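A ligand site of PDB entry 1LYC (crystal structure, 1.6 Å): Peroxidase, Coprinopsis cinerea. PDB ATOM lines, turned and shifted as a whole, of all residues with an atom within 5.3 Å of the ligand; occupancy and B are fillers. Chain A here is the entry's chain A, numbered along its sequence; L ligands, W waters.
NE2 of His 183 binds FE1 of the ligand, at 2.4 Å. An oxygen (O4) of the ligand is in salt-bridge range of the guanidinium group of Arg 47 (2.6 Å). O1 of the ligand sits at hydrogen-bond distance from N of Gly 190. N of Ser 187 lies within hydrogen-bond range of O4 of the ligand, at 3.0 Å. O4 of the ligand is in hydrogen-bond range of OG of Ser 187. An oxygen (O2) of the ligand lies within hydrogen-bond range of the backbone NH (N) of Glu 189 (2.9 Å). O1 of the ligand lies within hydrogen-bond range of N of Leu 191 (3.4 Å). The side-chain amino group (NZ) of Lys 48 lies within salt-bridge range of an oxygen (O3) of the ligand (3.98 Å).
CB of Leu 50 touches C31 of the ligand (3.4 Å). Arg 51 touches the ligand. CD2 of Phe 54 touches C24 of the ligand, at 3.5 Å. Pro 153 touches the ligand. Gly 154 touches the ligand. Pro 155 touches the ligand. Leu 179 touches the ligand. CD2 of Leu 180 touches C3 of the ligand, at 3.4 Å. CB of Ala 182 touches C26 of the ligand (3.6 Å). Leu 185 touches the ligand. CB of Ala 186 touches C32 of the ligand, 3.4 Å away. CA of Gln 188 touches O2 of the ligand, 3.7 Å away. SD of Met 242 touches C2 of the ligand (3.5 Å). OG of Ser 244 touches C17 of the ligand, at 3.5 Å. Tyr 272 touches the ligand (OH to C26, 3.98 Å). SD of Met 276 touches C26 of the ligand, at 3.5 Å. Within 4 Å of the ligand: Arg 47, Lys 48, Leu 50, Arg 51, Phe 54, Pro 153, Gly 154, Pro 155, Leu 179, Leu 180, Ala 182, His 183, Leu 185, Ala 186, Ser 187, Gln 188, Glu 189, Gly 190, Leu 191, Met 242, Ser 244, Tyr 272 and Met 276.
Water W1 lies within hydrogen-bond range of O3 of the ligand (2.6 Å), NZ of Lys 48 (2.8 Å) and NH1 of Arg 51 (2.8 Å). Water W3 lies within hydrogen-bond range of OG of Ser 44 (2.6 Å), OE2 of Glu 189 (2.8 Å), O3 of the ligand (2.9 Å) and NH2 of Arg 47 (3.1 Å). Water W4 lies within hydrogen-bond range of an oxygen (O2) of the ligand and the guanidinium group (NH1) of Arg 51.
N of Gly 190 is in hydrogen-bond range of OE1 of Gln 188, at 3.5 Å. OE1 of Glu 189 lies within salt-bridge range of NZ of Lys 48 (2.6 Å). N of Leu 191 lies within hydrogen-bond range of OE1 of Gln 188 (3.0 Å). The backbone NH (N) of Leu 200 lies within hydrogen-bond range of the backbone carbonyl oxygen (O) of Ala 186, 3.0 Å away. SD of Met 242 lies within hydrogen-bond range of OG of Ser 244 (3.5 Å).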
ATOM      1  N   SER A  44      10.353 -17.021  21.554  1.00  0.00           N
ATOM      2  CA  SER A  44      10.989 -16.403  20.388  1.00  0.00           C
ATOM      3  C   SER A  44      11.156 -17.304  19.161  1.00  0.00           C
ATOM      4  O   SER A  44      10.785 -16.907  18.055  1.00  0.00           O
ATOM      5  CB  SER A  44      12.348 -15.824  20.775  1.00  0.00           C
ATOM      6  OG  SER A  44      12.897 -15.098  19.690  1.00  0.00           O
ATOM      7  N   VAL A  46       9.519 -19.851  17.980  1.00  0.00           N
ATOM      8  CA  VAL A  46       8.262 -20.033  17.251  1.00  0.00           C
ATOM      9  C   VAL A  46       7.910 -18.762  16.484  1.00  0.00           C
ATOM     10  O   VAL A  46       7.447 -18.821  15.334  1.00  0.00           O
ATOM     11  CB  VAL A  46       7.102 -20.367  18.219  1.00  0.00           C
ATOM     12  CG1 VAL A  46       5.842 -20.706  17.428  1.00  0.00           C
ATOM     13  CG2 VAL A  46       7.480 -21.519  19.131  1.00  0.00           C
ATOM     14  N   ARG A  47       8.118 -17.606  17.105  1.00  0.00           N
ATOM     15  CA  ARG A  47       7.810 -16.335  16.467  1.00  0.00           C
ATOM     16  C   ARG A  47       8.775 -16.066  15.305  1.00  0.00           C
ATOM     17  O   ARG A  47       8.372 -15.619  14.225  1.00  0.00           O
ATOM     18  CB  ARG A  47       7.839 -15.206  17.508  1.00  0.00           C
ATOM     19  CG  ARG A  47       6.898 -15.436  18.691  1.00  0.00           C
ATOM     20  CD  ARG A  47       6.690 -14.182  19.512  1.00  0.00           C
ATOM     21  NE  ARG A  47       7.958 -13.655  20.039  1.00  0.00           N
ATOM     22  CZ  ARG A  47       8.513 -14.045  21.187  1.00  0.00           C
ATOM     23  NH1 ARG A  47       7.931 -14.966  21.957  1.00  0.00           N
ATOM     24  NH2 ARG A  47       9.665 -13.502  21.574  1.00  0.00           N
ATOM     25  N   LYS A  48      10.055 -16.372  15.522  1.00  0.00           N
ATOM     26  CA  LYS A  48      11.077 -16.207  14.491  1.00  0.00           C
ATOM     27  C   LYS A  48      10.782 -17.125  13.274  1.00  0.00           C
ATOM     28  O   LYS A  48      10.945 -16.723  12.116  1.00  0.00           O
ATOM     29  CB  LYS A  48      12.460 -16.551  15.044  1.00  0.00           C
ATOM     30  CG  LYS A  48      12.973 -15.594  16.110  1.00  0.00           C
ATOM     31  CD  LYS A  48      13.370 -14.241  15.523  1.00  0.00           C
ATOM     32  CE  LYS A  48      14.065 -13.377  16.581  1.00  0.00           C
ATOM     33  NZ  LYS A  48      14.335 -12.016  16.060  1.00  0.00           N
ATOM     34  N   LEU A  50       7.890 -18.180  12.338  1.00  0.00           N
ATOM     35  CA  LEU A  50       6.718 -17.704  11.628  1.00  0.00           C
ATOM     36  C   LEU A  50       7.104 -16.611  10.618  1.00  0.00           C
ATOM     37  O   LEU A  50       6.511 -16.510   9.552  1.00  0.00           O
ATOM     38  CB  LEU A  50       5.661 -17.192  12.611  1.00  0.00           C
ATOM     39  CG  LEU A  50       4.827 -18.265  13.311  1.00  0.00           C
ATOM     40  CD1 LEU A  50       3.953 -17.637  14.384  1.00  0.00           C
ATOM     41  CD2 LEU A  50       3.959 -18.987  12.281  1.00  0.00           C
ATOM     42  N   ARG A  51       8.102 -15.804  10.984  1.00  0.00           N
ATOM     43  CA  ARG A  51       8.600 -14.755  10.093  1.00  0.00           C
ATOM     44  C   ARG A  51       9.303 -15.433   8.908  1.00  0.00           C
ATOM     45  O   ARG A  51       9.160 -15.028   7.749  1.00  0.00           O
ATOM     46  CB  ARG A  51       9.600 -13.851  10.832  1.00  0.00           C
ATOM     47  CG  ARG A  51       8.987 -12.865  11.825  1.00  0.00           C
ATOM     48  CD  ARG A  51      10.050 -11.932  12.420  1.00  0.00           C
ATOM     49  NE  ARG A  51      10.746 -11.178  11.382  1.00  0.00           N
ATOM     50  CZ  ARG A  51      12.015 -10.773  11.456  1.00  0.00           C
ATOM     51  NH1 ARG A  51      12.737 -11.043  12.544  1.00  0.00           N
ATOM     52  NH2 ARG A  51      12.578 -10.119  10.444  1.00  0.00           N
ATOM     53  N   VAL A  53       8.853 -18.598   7.629  1.00  0.00           N
ATOM     54  CA  VAL A  53       7.944 -19.280   6.726  1.00  0.00           C
ATOM     55  C   VAL A  53       7.240 -18.288   5.793  1.00  0.00           C
ATOM     56  O   VAL A  53       7.039 -18.584   4.611  1.00  0.00           O
ATOM     57  CB  VAL A  53       6.888 -20.113   7.504  1.00  0.00           C
ATOM     58  CG1 VAL A  53       5.935 -19.202   8.279  1.00  0.00           C
ATOM     59  CG2 VAL A  53       6.132 -21.020   6.542  1.00  0.00           C
ATOM     60  N   PHE A  54       6.874 -17.124   6.310  1.00  0.00           N
ATOM     61  CA  PHE A  54       6.239 -16.099   5.477  1.00  0.00           C
ATOM     62  C   PHE A  54       7.245 -15.578   4.446  1.00  0.00           C
ATOM     63  O   PHE A  54       6.977 -15.565   3.249  1.00  0.00           O
ATOM     64  CB  PHE A  54       5.720 -14.934   6.334  1.00  0.00           C
ATOM     65  CG  PHE A  54       5.197 -13.754   5.520  1.00  0.00           C
ATOM     66  CD1 PHE A  54       5.565 -12.449   5.842  1.00  0.00           C
ATOM     67  CD2 PHE A  54       4.326 -13.958   4.437  1.00  0.00           C
ATOM     68  CE1 PHE A  54       5.077 -11.362   5.098  1.00  0.00           C
ATOM     69  CE2 PHE A  54       3.838 -12.871   3.693  1.00  0.00           C
ATOM     70  CZ  PHE A  54       4.214 -11.582   4.027  1.00  0.00           C
ATOM     71  N   PRO A 153       6.516  -7.769   1.753  1.00  0.00           N
ATOM     72  CA  PRO A 153       5.778  -6.550   2.134  1.00  0.00           C
ATOM     73  C   PRO A 153       6.328  -5.993   3.458  1.00  0.00           C
ATOM     74  O   PRO A 153       6.582  -6.758   4.404  1.00  0.00           O
ATOM     75  CB  PRO A 153       4.331  -7.041   2.260  1.00  0.00           C
ATOM     76  CG  PRO A 153       4.269  -8.167   1.297  1.00  0.00           C
ATOM     77  CD  PRO A 153       5.569  -8.896   1.565  1.00  0.00           C
ATOM     78  N   GLY A 154       6.496  -4.675   3.531  1.00  0.00           N
ATOM     79  CA  GLY A 154       7.025  -4.065   4.728  1.00  0.00           C
ATOM     80  C   GLY A 154       6.058  -3.183   5.515  1.00  0.00           C
ATOM     81  O   GLY A 154       5.000  -2.793   4.989  1.00  0.00           O
ATOM     82  N   PRO A 155       6.384  -2.879   6.782  1.00  0.00           N
ATOM     83  CA  PRO A 155       5.539  -2.035   7.641  1.00  0.00           C
ATOM     84  C   PRO A 155       5.491  -0.584   7.190  1.00  0.00           C
ATOM     85  O   PRO A 155       4.694   0.207   7.678  1.00  0.00           O
ATOM     86  CB  PRO A 155       6.174  -2.215   9.018  1.00  0.00           C
ATOM     87  CG  PRO A 155       7.614  -2.415   8.695  1.00  0.00           C
ATOM     88  CD  PRO A 155       7.545  -3.374   7.531  1.00  0.00           C
ATOM     89  N   ILE A 162       0.917  -3.402  -0.218  1.00  0.00           N
ATOM     90  CA  ILE A 162       0.811  -4.711   0.423  1.00  0.00           C
ATOM     91  C   ILE A 162      -0.185  -5.645  -0.276  1.00  0.00           C
ATOM     92  O   ILE A 162       0.118  -6.827  -0.481  1.00  0.00           O
ATOM     93  CB  ILE A 162       0.388  -4.557   1.891  1.00  0.00           C
ATOM     94  CG1 ILE A 162       1.505  -3.846   2.677  1.00  0.00           C
ATOM     95  CG2 ILE A 162       0.085  -5.925   2.494  1.00  0.00           C
ATOM     96  CD1 ILE A 162       1.131  -3.543   4.114  1.00  0.00           C
ATOM     97  N   MET A 166       0.789  -9.004  -2.319  1.00  0.00           N
ATOM     98  CA  MET A 166       0.181 -10.250  -1.845  1.00  0.00           C
ATOM     99  C   MET A 166      -0.804 -10.835  -2.867  1.00  0.00           C
ATOM    100  O   MET A 166      -0.920 -12.053  -2.994  1.00  0.00           O
ATOM    101  CB  MET A 166      -0.534 -10.008  -0.511  1.00  0.00           C
ATOM    102  CG  MET A 166       0.406  -9.662   0.652  1.00  0.00           C
ATOM    103  SD  MET A 166       1.460 -11.033   1.230  1.00  0.00           S
ATOM    104  CE  MET A 166       0.315 -11.917   2.282  1.00  0.00           C
ATOM    105  N   VAL A 176      -5.057 -11.947   3.171  1.00  0.00           N
ATOM    106  CA  VAL A 176      -3.944 -11.189   3.740  1.00  0.00           C
ATOM    107  C   VAL A 176      -4.242 -10.942   5.230  1.00  0.00           C
ATOM    108  O   VAL A 176      -3.368 -11.092   6.090  1.00  0.00           O
ATOM    109  CB  VAL A 176      -3.756  -9.853   3.013  1.00  0.00           C
ATOM    110  CG1 VAL A 176      -2.754  -8.963   3.771  1.00  0.00           C
ATOM    111  CG2 VAL A 176      -3.243 -10.114   1.598  1.00  0.00           C
ATOM    112  N   LEU A 179      -3.824 -14.342   7.254  1.00  0.00           N
ATOM    113  CA  LEU A 179      -2.439 -14.741   7.532  1.00  0.00           C
ATOM    114  C   LEU A 179      -1.880 -13.937   8.708  1.00  0.00           C
ATOM    115  O   LEU A 179      -1.037 -14.433   9.474  1.00  0.00           O
ATOM    116  CB  LEU A 179      -1.524 -14.512   6.314  1.00  0.00           C
ATOM    117  CG  LEU A 179      -1.235 -15.573   5.236  1.00  0.00           C
ATOM    118  CD1 LEU A 179      -0.962 -16.903   5.889  1.00  0.00           C
ATOM    119  CD2 LEU A 179      -2.391 -15.684   4.262  1.00  0.00           C
ATOM    120  N   LEU A 180      -2.347 -12.707   8.843  1.00  0.00           N
ATOM    121  CA  LEU A 180      -1.885 -11.822   9.916  1.00  0.00           C
ATOM    122  C   LEU A 180      -2.345 -12.210  11.330  1.00  0.00           C
ATOM    123  O   LEU A 180      -2.004 -11.544  12.316  1.00  0.00           O
ATOM    124  CB  LEU A 180      -2.267 -10.370   9.588  1.00  0.00           C
ATOM    125  CG  LEU A 180      -1.212  -9.685   8.708  1.00  0.00           C
ATOM    126  CD1 LEU A 180      -1.697  -8.349   8.184  1.00  0.00           C
ATOM    127  CD2 LEU A 180       0.065  -9.490   9.542  1.00  0.00           C
ATOM    128  N   ALA A 182      -1.170 -14.347  12.692  1.00  0.00           N
ATOM    129  CA  ALA A 182       0.136 -14.736  13.208  1.00  0.00           C
ATOM    130  C   ALA A 182       0.691 -13.690  14.188  1.00  0.00           C
ATOM    131  O   ALA A 182       1.505 -14.019  15.053  1.00  0.00           O
ATOM    132  CB  ALA A 182       1.113 -14.941  12.040  1.00  0.00           C
ATOM    133  N   HIS A 183       0.254 -12.435  14.035  1.00  0.00           N
ATOM    134  CA  HIS A 183       0.705 -11.367  14.923  1.00  0.00           C
ATOM    135  C   HIS A 183       0.091 -11.502  16.320  1.00  0.00           C
ATOM    136  O   HIS A 183       0.338 -10.671  17.205  1.00  0.00           O
ATOM    137  CB  HIS A 183       0.356  -9.996  14.341  1.00  0.00           C
ATOM    138  CG  HIS A 183       1.341  -9.505  13.315  1.00  0.00           C
ATOM    139  ND1 HIS A 183       1.360  -8.231  12.800  1.00  0.00           N
ATOM    140  CD2 HIS A 183       2.362 -10.158  12.717  1.00  0.00           C
ATOM    141  CE1 HIS A 183       2.355  -8.146  11.917  1.00  0.00           C
ATOM    142  NE2 HIS A 183       3.001  -9.292  11.838  1.00  0.00           N
ATOM    143  N   LEU A 185       0.858 -13.951  18.079  1.00  0.00           N
ATOM    144  CA  LEU A 185       1.990 -14.556  18.783  1.00  0.00           C
ATOM    145  C   LEU A 185       3.232 -13.815  18.266  1.00  0.00           C
ATOM    146  O   LEU A 185       4.101 -14.409  17.631  1.00  0.00           O
ATOM    147  CB  LEU A 185       2.092 -16.043  18.424  1.00  0.00           C
ATOM    148  CG  LEU A 185       0.878 -16.948  18.654  1.00  0.00           C
ATOM    149  CD1 LEU A 185       1.176 -18.354  18.140  1.00  0.00           C
ATOM    150  CD2 LEU A 185       0.523 -16.980  20.128  1.00  0.00           C
ATOM    151  N   ALA A 186       3.328 -12.517  18.579  1.00  0.00           N
ATOM    152  CA  ALA A 186       4.428 -11.717  18.060  1.00  0.00           C
ATOM    153  C   ALA A 186       4.869 -10.527  18.903  1.00  0.00           C
ATOM    154  O   ALA A 186       4.187 -10.101  19.823  1.00  0.00           O
ATOM    155  CB  ALA A 186       4.053 -11.231  16.672  1.00  0.00           C
ATOM    156  N   SER A 187       6.041  -9.998  18.552  1.00  0.00           N
ATOM    157  CA  SER A 187       6.629  -8.829  19.189  1.00  0.00           C
ATOM    158  C   SER A 187       7.579  -8.217  18.151  1.00  0.00           C
ATOM    159  O   SER A 187       7.702  -8.745  17.042  1.00  0.00           O
ATOM    160  CB  SER A 187       7.411  -9.219  20.458  1.00  0.00           C
ATOM    161  OG  SER A 187       8.660  -9.817  20.152  1.00  0.00           O
ATOM    162  N   GLN A 188       8.215  -7.102  18.486  1.00  0.00           N
ATOM    163  CA  GLN A 188       9.157  -6.495  17.563  1.00  0.00           C
ATOM    164  C   GLN A 188      10.478  -6.284  18.282  1.00  0.00           C
ATOM    165  O   GLN A 188      10.494  -5.989  19.471  1.00  0.00           O
ATOM    166  CB  GLN A 188       8.624  -5.163  17.000  1.00  0.00           C
ATOM    167  CG  GLN A 188       8.470  -4.021  17.992  1.00  0.00           C
ATOM    168  CD  GLN A 188       9.793  -3.405  18.432  1.00  0.00           C
ATOM    169  OE1 GLN A 188      10.771  -3.389  17.663  1.00  0.00           O
ATOM    170  NE2 GLN A 188       9.831  -2.872  19.646  1.00  0.00           N
ATOM    171  N   GLU A 189      11.579  -6.439  17.560  1.00  0.00           N
ATOM    172  CA  GLU A 189      12.905  -6.269  18.150  1.00  0.00           C
ATOM    173  C   GLU A 189      13.688  -5.191  17.432  1.00  0.00           C
ATOM    174  O   GLU A 189      14.512  -4.510  18.039  1.00  0.00           O
ATOM    175  CB  GLU A 189      13.697  -7.571  18.065  1.00  0.00           C
ATOM    176  CG  GLU A 189      12.996  -8.793  18.587  1.00  0.00           C
ATOM    177  CD  GLU A 189      13.937  -9.981  18.657  1.00  0.00           C
ATOM    178  OE1 GLU A 189      14.775 -10.107  17.749  1.00  0.00           O
ATOM    179  OE2 GLU A 189      13.835 -10.781  19.614  1.00  0.00           O
ATOM    180  N   GLY A 190      13.417  -5.031  16.135  1.00  0.00           N
ATOM    181  CA  GLY A 190      14.147  -4.049  15.350  1.00  0.00           C
ATOM    182  C   GLY A 190      13.456  -2.778  14.901  1.00  0.00           C
ATOM    183  O   GLY A 190      14.108  -1.884  14.371  1.00  0.00           O
ATOM    184  N   LEU A 191      12.151  -2.673  15.111  1.00  0.00           N
ATOM    185  CA  LEU A 191      11.436  -1.469  14.716  1.00  0.00           C
ATOM    186  C   LEU A 191      11.699  -0.334  15.696  1.00  0.00           C
ATOM    187  O   LEU A 191      11.824   0.833  15.300  1.00  0.00           O
ATOM    188  CB  LEU A 191       9.937  -1.740  14.614  1.00  0.00           C
ATOM    189  CG  LEU A 191       9.562  -2.746  13.517  1.00  0.00           C
ATOM    190  CD1 LEU A 191       8.049  -2.954  13.516  1.00  0.00           C
ATOM    191  CD2 LEU A 191      10.032  -2.223  12.163  1.00  0.00           C
ATOM    192  N   LEU A 200       2.753  -7.471  20.294  1.00  0.00           N
ATOM    193  CA  LEU A 200       1.853  -6.871  19.331  1.00  0.00           C
ATOM    194  C   LEU A 200       0.417  -6.973  19.854  1.00  0.00           C
ATOM    195  O   LEU A 200      -0.481  -6.293  19.374  1.00  0.00           O
ATOM    196  CB  LEU A 200       1.993  -7.545  17.959  1.00  0.00           C
ATOM    197  CG  LEU A 200       3.038  -6.957  17.007  1.00  0.00           C
ATOM    198  CD1 LEU A 200       4.301  -6.558  17.755  1.00  0.00           C
ATOM    199  CD2 LEU A 200       3.341  -7.966  15.924  1.00  0.00           C
ATOM    200  N   MET A 242       2.258  -1.597  14.864  1.00  0.00           N
ATOM    201  CA  MET A 242       2.920  -1.469  13.576  1.00  0.00           C
ATOM    202  C   MET A 242       2.027  -0.662  12.635  1.00  0.00           C
ATOM    203  O   MET A 242       0.816  -0.873  12.605  1.00  0.00           O
ATOM    204  CB  MET A 242       3.166  -2.876  13.031  1.00  0.00           C
ATOM    205  CG  MET A 242       4.165  -2.979  11.917  1.00  0.00           C
ATOM    206  SD  MET A 242       4.297  -4.706  11.429  1.00  0.00           S
ATOM    207  CE  MET A 242       4.746  -5.449  13.062  1.00  0.00           C
ATOM    208  N   SER A 244       1.560  -0.744   9.400  1.00  0.00           N
ATOM    209  CA  SER A 244       0.818  -1.542   8.416  1.00  0.00           C
ATOM    210  C   SER A 244      -0.403  -2.228   9.040  1.00  0.00           C
ATOM    211  O   SER A 244      -1.450  -2.360   8.389  1.00  0.00           O
ATOM    212  CB  SER A 244       1.726  -2.592   7.766  1.00  0.00           C
ATOM    213  OG  SER A 244       2.447  -3.328   8.742  1.00  0.00           O
ATOM    214  N   LEU A 248      -4.183  -1.556   7.916  1.00  0.00           N
ATOM    215  CA  LEU A 248      -4.956  -2.691   7.395  1.00  0.00           C
ATOM    216  C   LEU A 248      -6.258  -2.872   8.159  1.00  0.00           C
ATOM    217  O   LEU A 248      -7.272  -3.281   7.592  1.00  0.00           O
ATOM    218  CB  LEU A 248      -4.131  -3.966   7.462  1.00  0.00           C
ATOM    219  CG  LEU A 248      -3.024  -4.088   6.415  1.00  0.00           C
ATOM    220  CD1 LEU A 248      -2.081  -5.207   6.799  1.00  0.00           C
ATOM    221  CD2 LEU A 248      -3.633  -4.321   5.025  1.00  0.00           C
ATOM    222  N   TYR A 272      -7.062 -18.959   9.198  1.00  0.00           N
ATOM    223  CA  TYR A 272      -5.601 -18.909   9.203  1.00  0.00           C
ATOM    224  C   TYR A 272      -5.069 -20.204   8.595  1.00  0.00           C
ATOM    225  O   TYR A 272      -4.245 -20.168   7.668  1.00  0.00           O
ATOM    226  CB  TYR A 272      -5.115 -18.746  10.646  1.00  0.00           C
ATOM    227  CG  TYR A 272      -3.602 -18.764  10.862  1.00  0.00           C
ATOM    228  CD1 TYR A 272      -2.994 -19.828  11.538  1.00  0.00           C
ATOM    229  CD2 TYR A 272      -2.805 -17.693  10.451  1.00  0.00           C
ATOM    230  CE1 TYR A 272      -1.622 -19.828  11.818  1.00  0.00           C
ATOM    231  CE2 TYR A 272      -1.427 -17.686  10.720  1.00  0.00           C
ATOM    232  CZ  TYR A 272      -0.853 -18.748  11.407  1.00  0.00           C
ATOM    233  OH  TYR A 272       0.498 -18.727  11.690  1.00  0.00           O
ATOM    234  N   MET A 276      -2.630 -20.466   5.576  1.00  0.00           N
ATOM    235  CA  MET A 276      -1.315 -21.070   5.711  1.00  0.00           C
ATOM    236  C   MET A 276      -1.130 -22.245   4.741  1.00  0.00           C
ATOM    237  O   MET A 276      -0.036 -22.449   4.201  1.00  0.00           O
ATOM    238  CB  MET A 276      -1.090 -21.531   7.154  1.00  0.00           C
ATOM    239  CG  MET A 276      -0.904 -20.406   8.139  1.00  0.00           C
ATOM    240  SD  MET A 276       0.468 -19.312   7.702  1.00  0.00           S
ATOM    241  CE  MET A 276       1.847 -20.026   8.643  1.00  0.00           C
ATOM    242  N   MET A 279      -0.336 -20.797   1.392  1.00  0.00           N
ATOM    243  CA  MET A 279       1.033 -20.306   1.335  1.00  0.00           C
ATOM    244  C   MET A 279       2.082 -21.414   1.284  1.00  0.00           C
ATOM    245  O   MET A 279       3.132 -21.242   0.673  1.00  0.00           O
ATOM    246  CB  MET A 279       1.277 -19.385   2.535  1.00  0.00           C
ATOM    247  CG  MET A 279       2.512 -18.524   2.429  1.00  0.00           C
ATOM    248  SD  MET A 279       2.646 -17.254   3.740  1.00  0.00           S
ATOM    249  CE  MET A 279       3.448 -18.211   5.076  1.00  0.00           C
HETATM  250  C1  LIG L   1       6.949  -9.493  13.412  1.00  0.00           C
HETATM  251  C2  LIG L   1       5.737  -7.210   9.407  1.00  0.00           C
HETATM  252  C3  LIG L   1       2.790 -10.592   7.758  1.00  0.00           C
HETATM  253  C4  LIG L   1       4.598 -13.422  11.460  1.00  0.00           C
HETATM  254  C5  LIG L   1       7.048  -8.435  12.508  1.00  0.00           C
HETATM  255  C6  LIG L   1       7.855  -7.375  12.428  1.00  0.00           C
HETATM  256  C7  LIG L   1       7.589  -6.755  11.223  1.00  0.00           C
HETATM  257  C8  LIG L   1       6.421  -7.618  10.560  1.00  0.00           C
HETATM  258  C9  LIG L   1       8.239  -5.297  10.587  1.00  0.00           C
HETATM  259  C10 LIG L   1       8.879  -6.870  13.426  1.00  0.00           C
HETATM  260  C11 LIG L   1      10.299  -7.721  13.404  1.00  0.00           C
HETATM  261  C12 LIG L   1      11.246  -7.181  14.355  1.00  0.00           C
HETATM  262  O1  LIG L   1      11.493  -5.910  14.441  1.00  0.00           O
HETATM  263  O2  LIG L   1      11.488  -8.127  15.226  1.00  0.00           O
HETATM  264  C13 LIG L   1       4.768  -7.717   8.627  1.00  0.00           C
HETATM  265  C14 LIG L   1       4.091  -7.061   7.432  1.00  0.00           C
HETATM  266  C15 LIG L   1       3.138  -8.146   6.947  1.00  0.00           C
HETATM  267  C16 LIG L   1       3.331  -9.237   7.728  1.00  0.00           C
HETATM  268  C17 LIG L   1       4.215  -5.710   6.887  1.00  0.00           C
HETATM  269  C18 LIG L   1       1.989  -7.911   5.608  1.00  0.00           C
HETATM  270  C19 LIG L   1       1.076  -8.873   5.079  1.00  0.00           C
HETATM  271  C20 LIG L   1       3.018 -11.683   8.408  1.00  0.00           C
HETATM  272  C21 LIG L   1       2.656 -13.128   8.040  1.00  0.00           C
HETATM  273  C22 LIG L   1       3.297 -14.163   9.107  1.00  0.00           C
HETATM  274  C23 LIG L   1       4.011 -13.078  10.167  1.00  0.00           C
HETATM  275  C24 LIG L   1       1.721 -13.425   6.733  1.00  0.00           C
HETATM  276  C25 LIG L   1       3.222 -15.559   9.174  1.00  0.00           C
HETATM  277  C26 LIG L   1       1.960 -16.357   8.853  1.00  0.00           C
HETATM  278  C27 LIG L   1       5.237 -12.573  12.343  1.00  0.00           C
HETATM  279  C28 LIG L   1       5.668 -13.050  13.721  1.00  0.00           C
HETATM  280  C29 LIG L   1       6.490 -11.885  14.234  1.00  0.00           C
HETATM  281  C30 LIG L   1       6.357 -10.869  13.312  1.00  0.00           C
HETATM  282  C31 LIG L   1       5.315 -14.422  14.511  1.00  0.00           C
HETATM  283  C32 LIG L   1       7.212 -11.911  15.596  1.00  0.00           C
HETATM  284  C33 LIG L   1       8.477 -12.004  15.657  1.00  0.00           C
HETATM  285  C34 LIG L   1       9.224 -11.933  17.157  1.00  0.00           C
HETATM  286  O3  LIG L   1      10.493 -11.914  17.106  1.00  0.00           O
HETATM  287  O4  LIG L   1       8.453 -11.844  18.277  1.00  0.00           O
HETATM  288  N1  LIG L   1       6.175  -8.545  11.223  1.00  0.00           N
HETATM  289  N2  LIG L   1       4.332  -8.880   8.859  1.00  0.00           N
HETATM  290  N3  LIG L   1       3.840 -11.673   9.709  1.00  0.00           N
HETATM  291  N4  LIG L   1       5.600 -11.218  12.194  1.00  0.00           N
HETATM  292 FE1  LIG L   1       4.884 -10.052  10.586  1.00  0.00          FE
HETATM  293  O   HOH W   1      11.966 -10.836  15.227  1.00  0.00           O
HETATM  294  O   HOH W   2       9.820  -8.842   9.740  1.00  0.00           O
HETATM  295  O   HOH W   3      11.823 -12.768  19.526  1.00  0.00           O
HETATM  296  O   HOH W   4      14.355  -8.561  14.182  1.00  0.00           O
HETATM  297  O   HOH W   5       1.381  -5.850   8.664  1.00  0.00           O
